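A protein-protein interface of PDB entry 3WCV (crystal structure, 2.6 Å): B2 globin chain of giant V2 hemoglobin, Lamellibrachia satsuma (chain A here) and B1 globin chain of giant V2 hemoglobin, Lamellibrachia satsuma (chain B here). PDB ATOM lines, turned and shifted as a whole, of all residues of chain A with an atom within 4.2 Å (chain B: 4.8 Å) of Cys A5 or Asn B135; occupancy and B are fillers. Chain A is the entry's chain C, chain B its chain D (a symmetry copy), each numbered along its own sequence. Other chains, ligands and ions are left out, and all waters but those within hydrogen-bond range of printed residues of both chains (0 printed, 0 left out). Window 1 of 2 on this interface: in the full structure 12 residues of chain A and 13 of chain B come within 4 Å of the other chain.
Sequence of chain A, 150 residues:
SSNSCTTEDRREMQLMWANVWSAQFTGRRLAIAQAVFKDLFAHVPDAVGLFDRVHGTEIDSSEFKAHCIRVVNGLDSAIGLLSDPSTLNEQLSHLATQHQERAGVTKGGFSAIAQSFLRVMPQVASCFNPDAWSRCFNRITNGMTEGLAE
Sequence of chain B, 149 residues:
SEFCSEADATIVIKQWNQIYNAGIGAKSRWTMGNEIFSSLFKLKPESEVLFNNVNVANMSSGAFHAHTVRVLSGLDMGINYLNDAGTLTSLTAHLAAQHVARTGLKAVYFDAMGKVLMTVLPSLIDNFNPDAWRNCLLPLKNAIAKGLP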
ATOM      1  N   SER A   1     -21.091  23.305  10.704  1.00  0.00           N
ATOM      2  CA  SER A   1     -20.543  22.009  11.057  1.00  0.00           C
ATOM      3  C   SER A   1     -19.000  22.074  11.316  1.00  0.00           C
ATOM      4  O   SER A   1     -18.503  23.164  11.693  1.00  0.00           O
ATOM      5  CB  SER A   1     -20.896  21.071   9.920  1.00  0.00           C
ATOM      6  OG  SER A   1     -22.241  20.615   9.972  1.00  0.00           O
ATOM      7  N   ASN A   3     -18.538  19.088  12.989  1.00  0.00           N
ATOM      8  CA  ASN A   3     -18.624  18.187  14.078  1.00  0.00           C
ATOM      9  C   ASN A   3     -19.990  18.345  14.798  1.00  0.00           C
ATOM     10  O   ASN A   3     -20.176  18.096  16.020  1.00  0.00           O
ATOM     11  CB  ASN A   3     -17.516  18.324  15.154  1.00  0.00           C
ATOM     12  CG  ASN A   3     -16.381  17.477  14.798  1.00  0.00           C
ATOM     13  OD1 ASN A   3     -16.464  16.280  14.928  1.00  0.00           O
ATOM     14  ND2 ASN A   3     -15.242  18.103  14.441  1.00  0.00           N
ATOM     15  N   SER A   4     -20.970  18.879  14.058  1.00  0.00           N
ATOM     16  CA  SER A   4     -22.279  19.098  14.641  1.00  0.00           C
ATOM     17  C   SER A   4     -23.057  17.823  14.966  1.00  0.00           C
ATOM     18  O   SER A   4     -22.885  16.775  14.328  1.00  0.00           O
ATOM     19  CB  SER A   4     -23.108  19.969  13.709  1.00  0.00           C
ATOM     20  OG  SER A   4     -22.522  21.230  13.425  1.00  0.00           O
ATOM     21  N   CYS A   5     -23.949  17.933  15.947  1.00  0.00           N
ATOM     22  CA  CYS A   5     -24.803  16.813  16.319  1.00  0.00           C
ATOM     23  C   CYS A   5     -25.943  16.774  15.307  1.00  0.00           C
ATOM     24  O   CYS A   5     -26.875  17.559  15.388  1.00  0.00           O
ATOM     25  CB  CYS A   5     -25.350  16.995  17.743  1.00  0.00           C
ATOM     26  SG  CYS A   5     -26.674  15.825  18.218  1.00  0.00           S
ATOM     27  N   THR A   6     -25.865  15.840  14.359  1.00  0.00           N
ATOM     28  CA  THR A   6     -26.869  15.735  13.308  1.00  0.00           C
ATOM     29  C   THR A   6     -28.112  14.959  13.696  1.00  0.00           C
ATOM     30  O   THR A   6     -28.152  14.291  14.726  1.00  0.00           O
ATOM     31  CB  THR A   6     -26.294  15.059  12.054  1.00  0.00           C
ATOM     32  OG1 THR A   6     -26.158  13.653  12.297  1.00  0.00           O
ATOM     33  CG2 THR A   6     -24.929  15.648  11.702  1.00  0.00           C
ATOM     34  N   ARG A  10     -28.338  11.905  16.443  1.00  0.00           N
ATOM     35  CA  ARG A  10     -29.314  11.944  17.525  1.00  0.00           C
ATOM     36  C   ARG A  10     -30.109  10.652  17.581  1.00  0.00           C
ATOM     37  O   ARG A  10     -30.318  10.108  18.660  1.00  0.00           O
ATOM     38  CB  ARG A  10     -30.256  13.132  17.332  1.00  0.00           C
ATOM     39  CG  ARG A  10     -29.543  14.451  17.509  1.00  0.00           C
ATOM     40  CD  ARG A  10     -30.272  15.635  16.889  1.00  0.00           C
ATOM     41  NE  ARG A  10     -29.330  16.746  16.755  1.00  0.00           N
ATOM     42  CZ  ARG A  10     -29.430  17.911  17.392  1.00  0.00           C
ATOM     43  NH1 ARG A  10     -30.457  18.130  18.208  1.00  0.00           N
ATOM     44  NH2 ARG A  10     -28.481  18.835  17.236  1.00  0.00           N
ATOM     45  N   LEU A  82     -33.273  15.788  22.148  1.00  0.00           N
ATOM     46  CA  LEU A  82     -32.428  16.110  20.995  1.00  0.00           C
ATOM     47  C   LEU A  82     -33.346  16.189  19.770  1.00  0.00           C
ATOM     48  O   LEU A  82     -33.022  16.843  18.786  1.00  0.00           O
ATOM     49  CB  LEU A  82     -31.353  15.035  20.784  1.00  0.00           C
ATOM     50  CG  LEU A  82     -30.125  15.073  21.705  1.00  0.00           C
ATOM     51  CD1 LEU A  82     -29.292  13.815  21.571  1.00  0.00           C
ATOM     52  CD2 LEU A  82     -29.279  16.287  21.345  1.00  0.00           C
ATOM     53  N   ARG A 135     -20.378  13.697  19.640  1.00  0.00           N
ATOM     54  CA  ARG A 135     -20.851  14.890  18.954  1.00  0.00           C
ATOM     55  C   ARG A 135     -22.120  15.431  19.604  1.00  0.00           C
ATOM     56  O   ARG A 135     -22.282  16.637  19.743  1.00  0.00           O
ATOM     57  CB  ARG A 135     -21.085  14.628  17.461  1.00  0.00           C
ATOM     58  CG  ARG A 135     -19.807  14.638  16.623  1.00  0.00           C
ATOM     59  CD  ARG A 135     -20.118  14.748  15.142  1.00  0.00           C
ATOM     60  NE  ARG A 135     -20.754  13.538  14.620  1.00  0.00           N
ATOM     61  CZ  ARG A 135     -20.086  12.441  14.276  1.00  0.00           C
ATOM     62  NH1 ARG A 135     -20.741  11.388  13.814  1.00  0.00           N
ATOM     63  NH2 ARG A 135     -18.758  12.413  14.380  1.00  0.00           N
ATOM     64  N   CYS A 136     -23.015  14.554  20.030  1.00  0.00           N
ATOM     65  CA  CYS A 136     -24.242  15.025  20.659  1.00  0.00           C
ATOM     66  C   CYS A 136     -24.109  15.249  22.170  1.00  0.00           C
ATOM     67  O   CYS A 136     -24.852  16.032  22.760  1.00  0.00           O
ATOM     68  CB  CYS A 136     -25.382  14.055  20.343  1.00  0.00           C
ATOM     69  SG  CYS A 136     -25.742  14.038  18.557  1.00  0.00           S
ATOM     70  N   ARG A 139     -22.856  18.681  22.216  1.00  0.00           N
ATOM     71  CA  ARG A 139     -23.958  19.586  21.907  1.00  0.00           C
ATOM     72  C   ARG A 139     -24.763  19.832  23.186  1.00  0.00           C
ATOM     73  O   ARG A 139     -25.226  20.944  23.440  1.00  0.00           O
ATOM     74  CB  ARG A 139     -24.873  18.955  20.848  1.00  0.00           C
ATOM     75  CG  ARG A 139     -26.290  19.540  20.804  1.00  0.00           C
ATOM     76  CD  ARG A 139     -26.310  20.931  20.184  1.00  0.00           C
ATOM     77  NE  ARG A 139     -27.635  21.549  20.278  1.00  0.00           N
ATOM     78  CZ  ARG A 139     -28.118  22.151  21.360  1.00  0.00           C
ATOM     79  NH1 ARG A 139     -27.394  22.232  22.467  1.00  0.00           N
ATOM     80  NH2 ARG A 139     -29.330  22.683  21.335  1.00  0.00           N
ATOM     81  N   PHE B   3     -21.118  21.001   4.410  1.00  0.00           N
ATOM     82  CA  PHE B   3     -22.309  21.758   4.791  1.00  0.00           C
ATOM     83  C   PHE B   3     -23.067  21.210   5.987  1.00  0.00           C
ATOM     84  O   PHE B   3     -22.649  21.400   7.130  1.00  0.00           O
ATOM     85  CB  PHE B   3     -23.271  21.863   3.615  1.00  0.00           C
ATOM     86  CG  PHE B   3     -22.987  23.024   2.728  1.00  0.00           C
ATOM     87  CD1 PHE B   3     -22.309  22.856   1.533  1.00  0.00           C
ATOM     88  CD2 PHE B   3     -23.347  24.306   3.122  1.00  0.00           C
ATOM     89  CE1 PHE B   3     -21.988  23.952   0.746  1.00  0.00           C
ATOM     90  CE2 PHE B   3     -23.028  25.403   2.344  1.00  0.00           C
ATOM     91  CZ  PHE B   3     -22.347  25.227   1.155  1.00  0.00           C
ATOM     92  N   CYS B   4     -24.203  20.567   5.724  1.00  0.00           N
ATOM     93  CA  CYS B   4     -25.008  19.982   6.784  1.00  0.00           C
ATOM     94  C   CYS B   4     -25.562  18.630   6.350  1.00  0.00           C
ATOM     95  O   CYS B   4     -25.729  18.366   5.163  1.00  0.00           O
ATOM     96  CB  CYS B   4     -26.155  20.918   7.207  1.00  0.00           C
ATOM     97  SG  CYS B   4     -27.600  21.049   6.094  1.00  0.00           S
ATOM     98  N   ASP B   8     -30.656  16.593   8.305  1.00  0.00           N
ATOM     99  CA  ASP B   8     -30.870  17.977   8.743  1.00  0.00           C
ATOM    100  C   ASP B   8     -31.473  18.800   7.605  1.00  0.00           C
ATOM    101  O   ASP B   8     -32.515  19.457   7.771  1.00  0.00           O
ATOM    102  CB  ASP B   8     -29.549  18.617   9.194  1.00  0.00           C
ATOM    103  CG  ASP B   8     -29.050  18.073  10.529  1.00  0.00           C
ATOM    104  OD1 ASP B   8     -27.863  18.287  10.857  1.00  0.00           O
ATOM    105  OD2 ASP B   8     -29.849  17.437  11.254  1.00  0.00           O
ATOM    106  N   ASP B 131     -31.658  23.721  15.899  1.00  0.00           N
ATOM    107  CA  ASP B 131     -30.422  23.000  15.651  1.00  0.00           C
ATOM    108  C   ASP B 131     -30.254  22.624  14.188  1.00  0.00           C
ATOM    109  O   ASP B 131     -29.213  22.897  13.580  1.00  0.00           O
ATOM    110  CB  ASP B 131     -30.349  21.748  16.529  1.00  0.00           C
ATOM    111  CG  ASP B 131     -30.054  22.082  17.994  1.00  0.00           C
ATOM    112  OD1 ASP B 131     -29.834  21.146  18.793  1.00  0.00           O
ATOM    113  OD2 ASP B 131     -30.039  23.288  18.340  1.00  0.00           O
ATOM    114  N   ALA B 132     -31.272  22.003  13.615  1.00  0.00           N
ATOM    115  CA  ALA B 132     -31.179  21.603  12.221  1.00  0.00           C
ATOM    116  C   ALA B 132     -30.937  22.832  11.352  1.00  0.00           C
ATOM    117  O   ALA B 132     -30.205  22.774  10.355  1.00  0.00           O
ATOM    118  CB  ALA B 132     -32.446  20.901  11.791  1.00  0.00           C
ATOM    119  N   TRP B 133     -31.557  23.950  11.724  1.00  0.00           N
ATOM    120  CA  TRP B 133     -31.377  25.168  10.953  1.00  0.00           C
ATOM    121  C   TRP B 133     -29.960  25.700  11.130  1.00  0.00           C
ATOM    122  O   TRP B 133     -29.306  26.047  10.151  1.00  0.00           O
ATOM    123  CB  TRP B 133     -32.418  26.228  11.337  1.00  0.00           C
ATOM    124  CG  TRP B 133     -33.727  26.067  10.617  1.00  0.00           C
ATOM    125  CD1 TRP B 133     -34.779  25.300  11.005  1.00  0.00           C
ATOM    126  CD2 TRP B 133     -34.115  26.689   9.380  1.00  0.00           C
ATOM    127  NE1 TRP B 133     -35.808  25.404  10.093  1.00  0.00           N
ATOM    128  CE2 TRP B 133     -35.430  26.251   9.085  1.00  0.00           C
ATOM    129  CE3 TRP B 133     -33.481  27.572   8.492  1.00  0.00           C
ATOM    130  CZ2 TRP B 133     -36.127  26.663   7.944  1.00  0.00           C
ATOM    131  CZ3 TRP B 133     -34.178  27.986   7.344  1.00  0.00           C
ATOM    132  CH2 TRP B 133     -35.491  27.526   7.087  1.00  0.00           C
ATOM    133  N   ARG B 134     -29.478  25.746  12.368  1.00  0.00           N
ATOM    134  CA  ARG B 134     -28.122  26.227  12.626  1.00  0.00           C
ATOM    135  C   ARG B 134     -27.111  25.426  11.822  1.00  0.00           C
ATOM    136  O   ARG B 134     -26.287  25.985  11.109  1.00  0.00           O
ATOM    137  CB  ARG B 134     -27.783  26.137  14.121  1.00  0.00           C
ATOM    138  CG  ARG B 134     -28.311  27.314  14.925  1.00  0.00           C
ATOM    139  CD  ARG B 134     -28.421  27.023  16.417  1.00  0.00           C
ATOM    140  NE  ARG B 134     -29.233  28.038  17.095  1.00  0.00           N
ATOM    141  CZ  ARG B 134     -29.988  27.810  18.170  1.00  0.00           C
ATOM    142  NH1 ARG B 134     -30.053  26.588  18.709  1.00  0.00           N
ATOM    143  NH2 ARG B 134     -30.697  28.803  18.705  1.00  0.00           N
ATOM    144  N   ASN B 135     -27.196  24.109  11.935  1.00  0.00           N
ATOM    145  CA  ASN B 135     -26.292  23.211  11.236  1.00  0.00           C
ATOM    146  C   ASN B 135     -26.286  23.417   9.737  1.00  0.00           C
ATOM    147  O   ASN B 135     -25.270  23.189   9.098  1.00  0.00           O
ATOM    148  CB  ASN B 135     -26.654  21.759  11.536  1.00  0.00           C
ATOM    149  CG  ASN B 135     -26.480  21.412  12.994  1.00  0.00           C
ATOM    150  OD1 ASN B 135     -25.852  22.159  13.757  1.00  0.00           O
ATOM    151  ND2 ASN B 135     -27.017  20.269  13.394  1.00  0.00           N
ATOM    152  N   CYS B 136     -27.414  23.840   9.172  1.00  0.00           N
ATOM    153  CA  CYS B 136     -27.494  24.051   7.732  1.00  0.00           C
ATOM    154  C   CYS B 136     -27.260  25.487   7.305  1.00  0.00           C
ATOM    155  O   CYS B 136     -26.688  25.736   6.251  1.00  0.00           O
ATOM    156  CB  CYS B 136     -28.851  23.594   7.211  1.00  0.00           C
ATOM    157  SG  CYS B 136     -29.066  21.797   7.300  1.00  0.00           S
ATOM    158  N   LEU B 137     -27.704  26.430   8.112  1.00  0.00           N
ATOM    159  CA  LEU B 137     -27.533  27.837   7.781  1.00  0.00           C
ATOM    160  C   LEU B 137     -26.159  28.414   8.025  1.00  0.00           C
ATOM    161  O   LEU B 137     -25.585  29.061   7.152  1.00  0.00           O
ATOM    162  CB  LEU B 137     -28.508  28.700   8.578  1.00  0.00           C
ATOM    163  CG  LEU B 137     -29.954  28.750   8.138  1.00  0.00           C
ATOM    164  CD1 LEU B 137     -30.574  30.018   8.733  1.00  0.00           C
ATOM    165  CD2 LEU B 137     -30.048  28.785   6.628  1.00  0.00           C
ATOM    166  N   PRO B 139     -23.209  27.215   8.013  1.00  0.00           N
ATOM    167  CA  PRO B 139     -22.258  26.921   6.931  1.00  0.00           C
ATOM    168  C   PRO B 139     -22.504  27.838   5.736  1.00  0.00           C
ATOM    169  O   PRO B 139     -21.550  28.389   5.142  1.00  0.00           O
ATOM    170  CB  PRO B 139     -22.523  25.451   6.622  1.00  0.00           C
ATOM    171  CG  PRO B 139     -22.926  24.920   7.999  1.00  0.00           C
ATOM    172  CD  PRO B 139     -23.862  25.986   8.496  1.00  0.00           C
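NH2 of Arg A10 sits at hydrogen-bond distance from O of Cys A5 (2.8 Å). SG of Cys A5 forms a disulfide with SG of Cys A136, at 2.0 Å. The backbone carbonyl oxygen of Thr A6 lies close to the guanidinium group of Arg A10 (3.4 Å). The backbone carbonyl oxygen (O) of Leu A82 sits at hydrogen-bond distance from the guanidinium group (NH1) of Arg A10. The side-chain amide nitrogen (ND2) of Asn B135 is in hydrogen-bond range of the side-chain carboxylate (OD1) of Asp B8. NH1 of Arg B134 lies within salt-bridge range of OD2 of Asp B131.
The backbone carbonyl oxygen of Phe B3 is in hydrogen-bond range of the side-chain hydroxyl of Ser A1, at 3.0 Å. The side-chain amide oxygen (OD1) of Asn B135 sits at hydrogen-bond distance from the side-chain hydroxyl (OG) of Ser A4 (3.5 Å). The backbone carbonyl oxygen of Cys A5 sits at hydrogen-bond distance from the side-chain amide nitrogen of Asn B135 (3.4 Å). The guanidinium group (NH2) of Arg A10 is in salt-bridge range of the side-chain carboxylate (OD1) of Asp B131 (3.1 Å). OD1 of Asp B131 is in salt-bridge range of NE of Arg A139 (2.7 Å).
Of the 11 printed residues of chain B, 5 touch a printed residue of chain A. Hydrophobic or aromatic side chains of chain B that line the printed part of chain A: Pro B139. Among the printed residues, 7 pairs touch across the chains. Among the printed residues, Asp or Glu carboxylates within 4 Å of a Lys or Arg side-chain nitrogen of the other chain: Arg A10 with Asp B131 and Arg A139 with Asp B131.
Ser A1 touches Pro B139 (N to CG, 3.6 Å). Asp B8 touches Thr A6 (OD1 to CA, 3.7 Å).
Printed residues of chain B within 4 Å of Ser A1: Phe B3 (3.0 Å) and Pro B139 (3.6 Å). Cys A5 touches just one residue of chain B: Asn B135 (3.4 Å). Of the printed residues of chain B, Thr A6 touches Asp B8. Arg A135 touches none of the printed residues of chain B. Of chain A, only Ser A4 (3.5 Å) and Cys A5 (3.4 Å) come within 4 Å of Asn B135. The nearest residue of chain B that does not touch Cys A5 is Asp B8 (4.7 Å).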
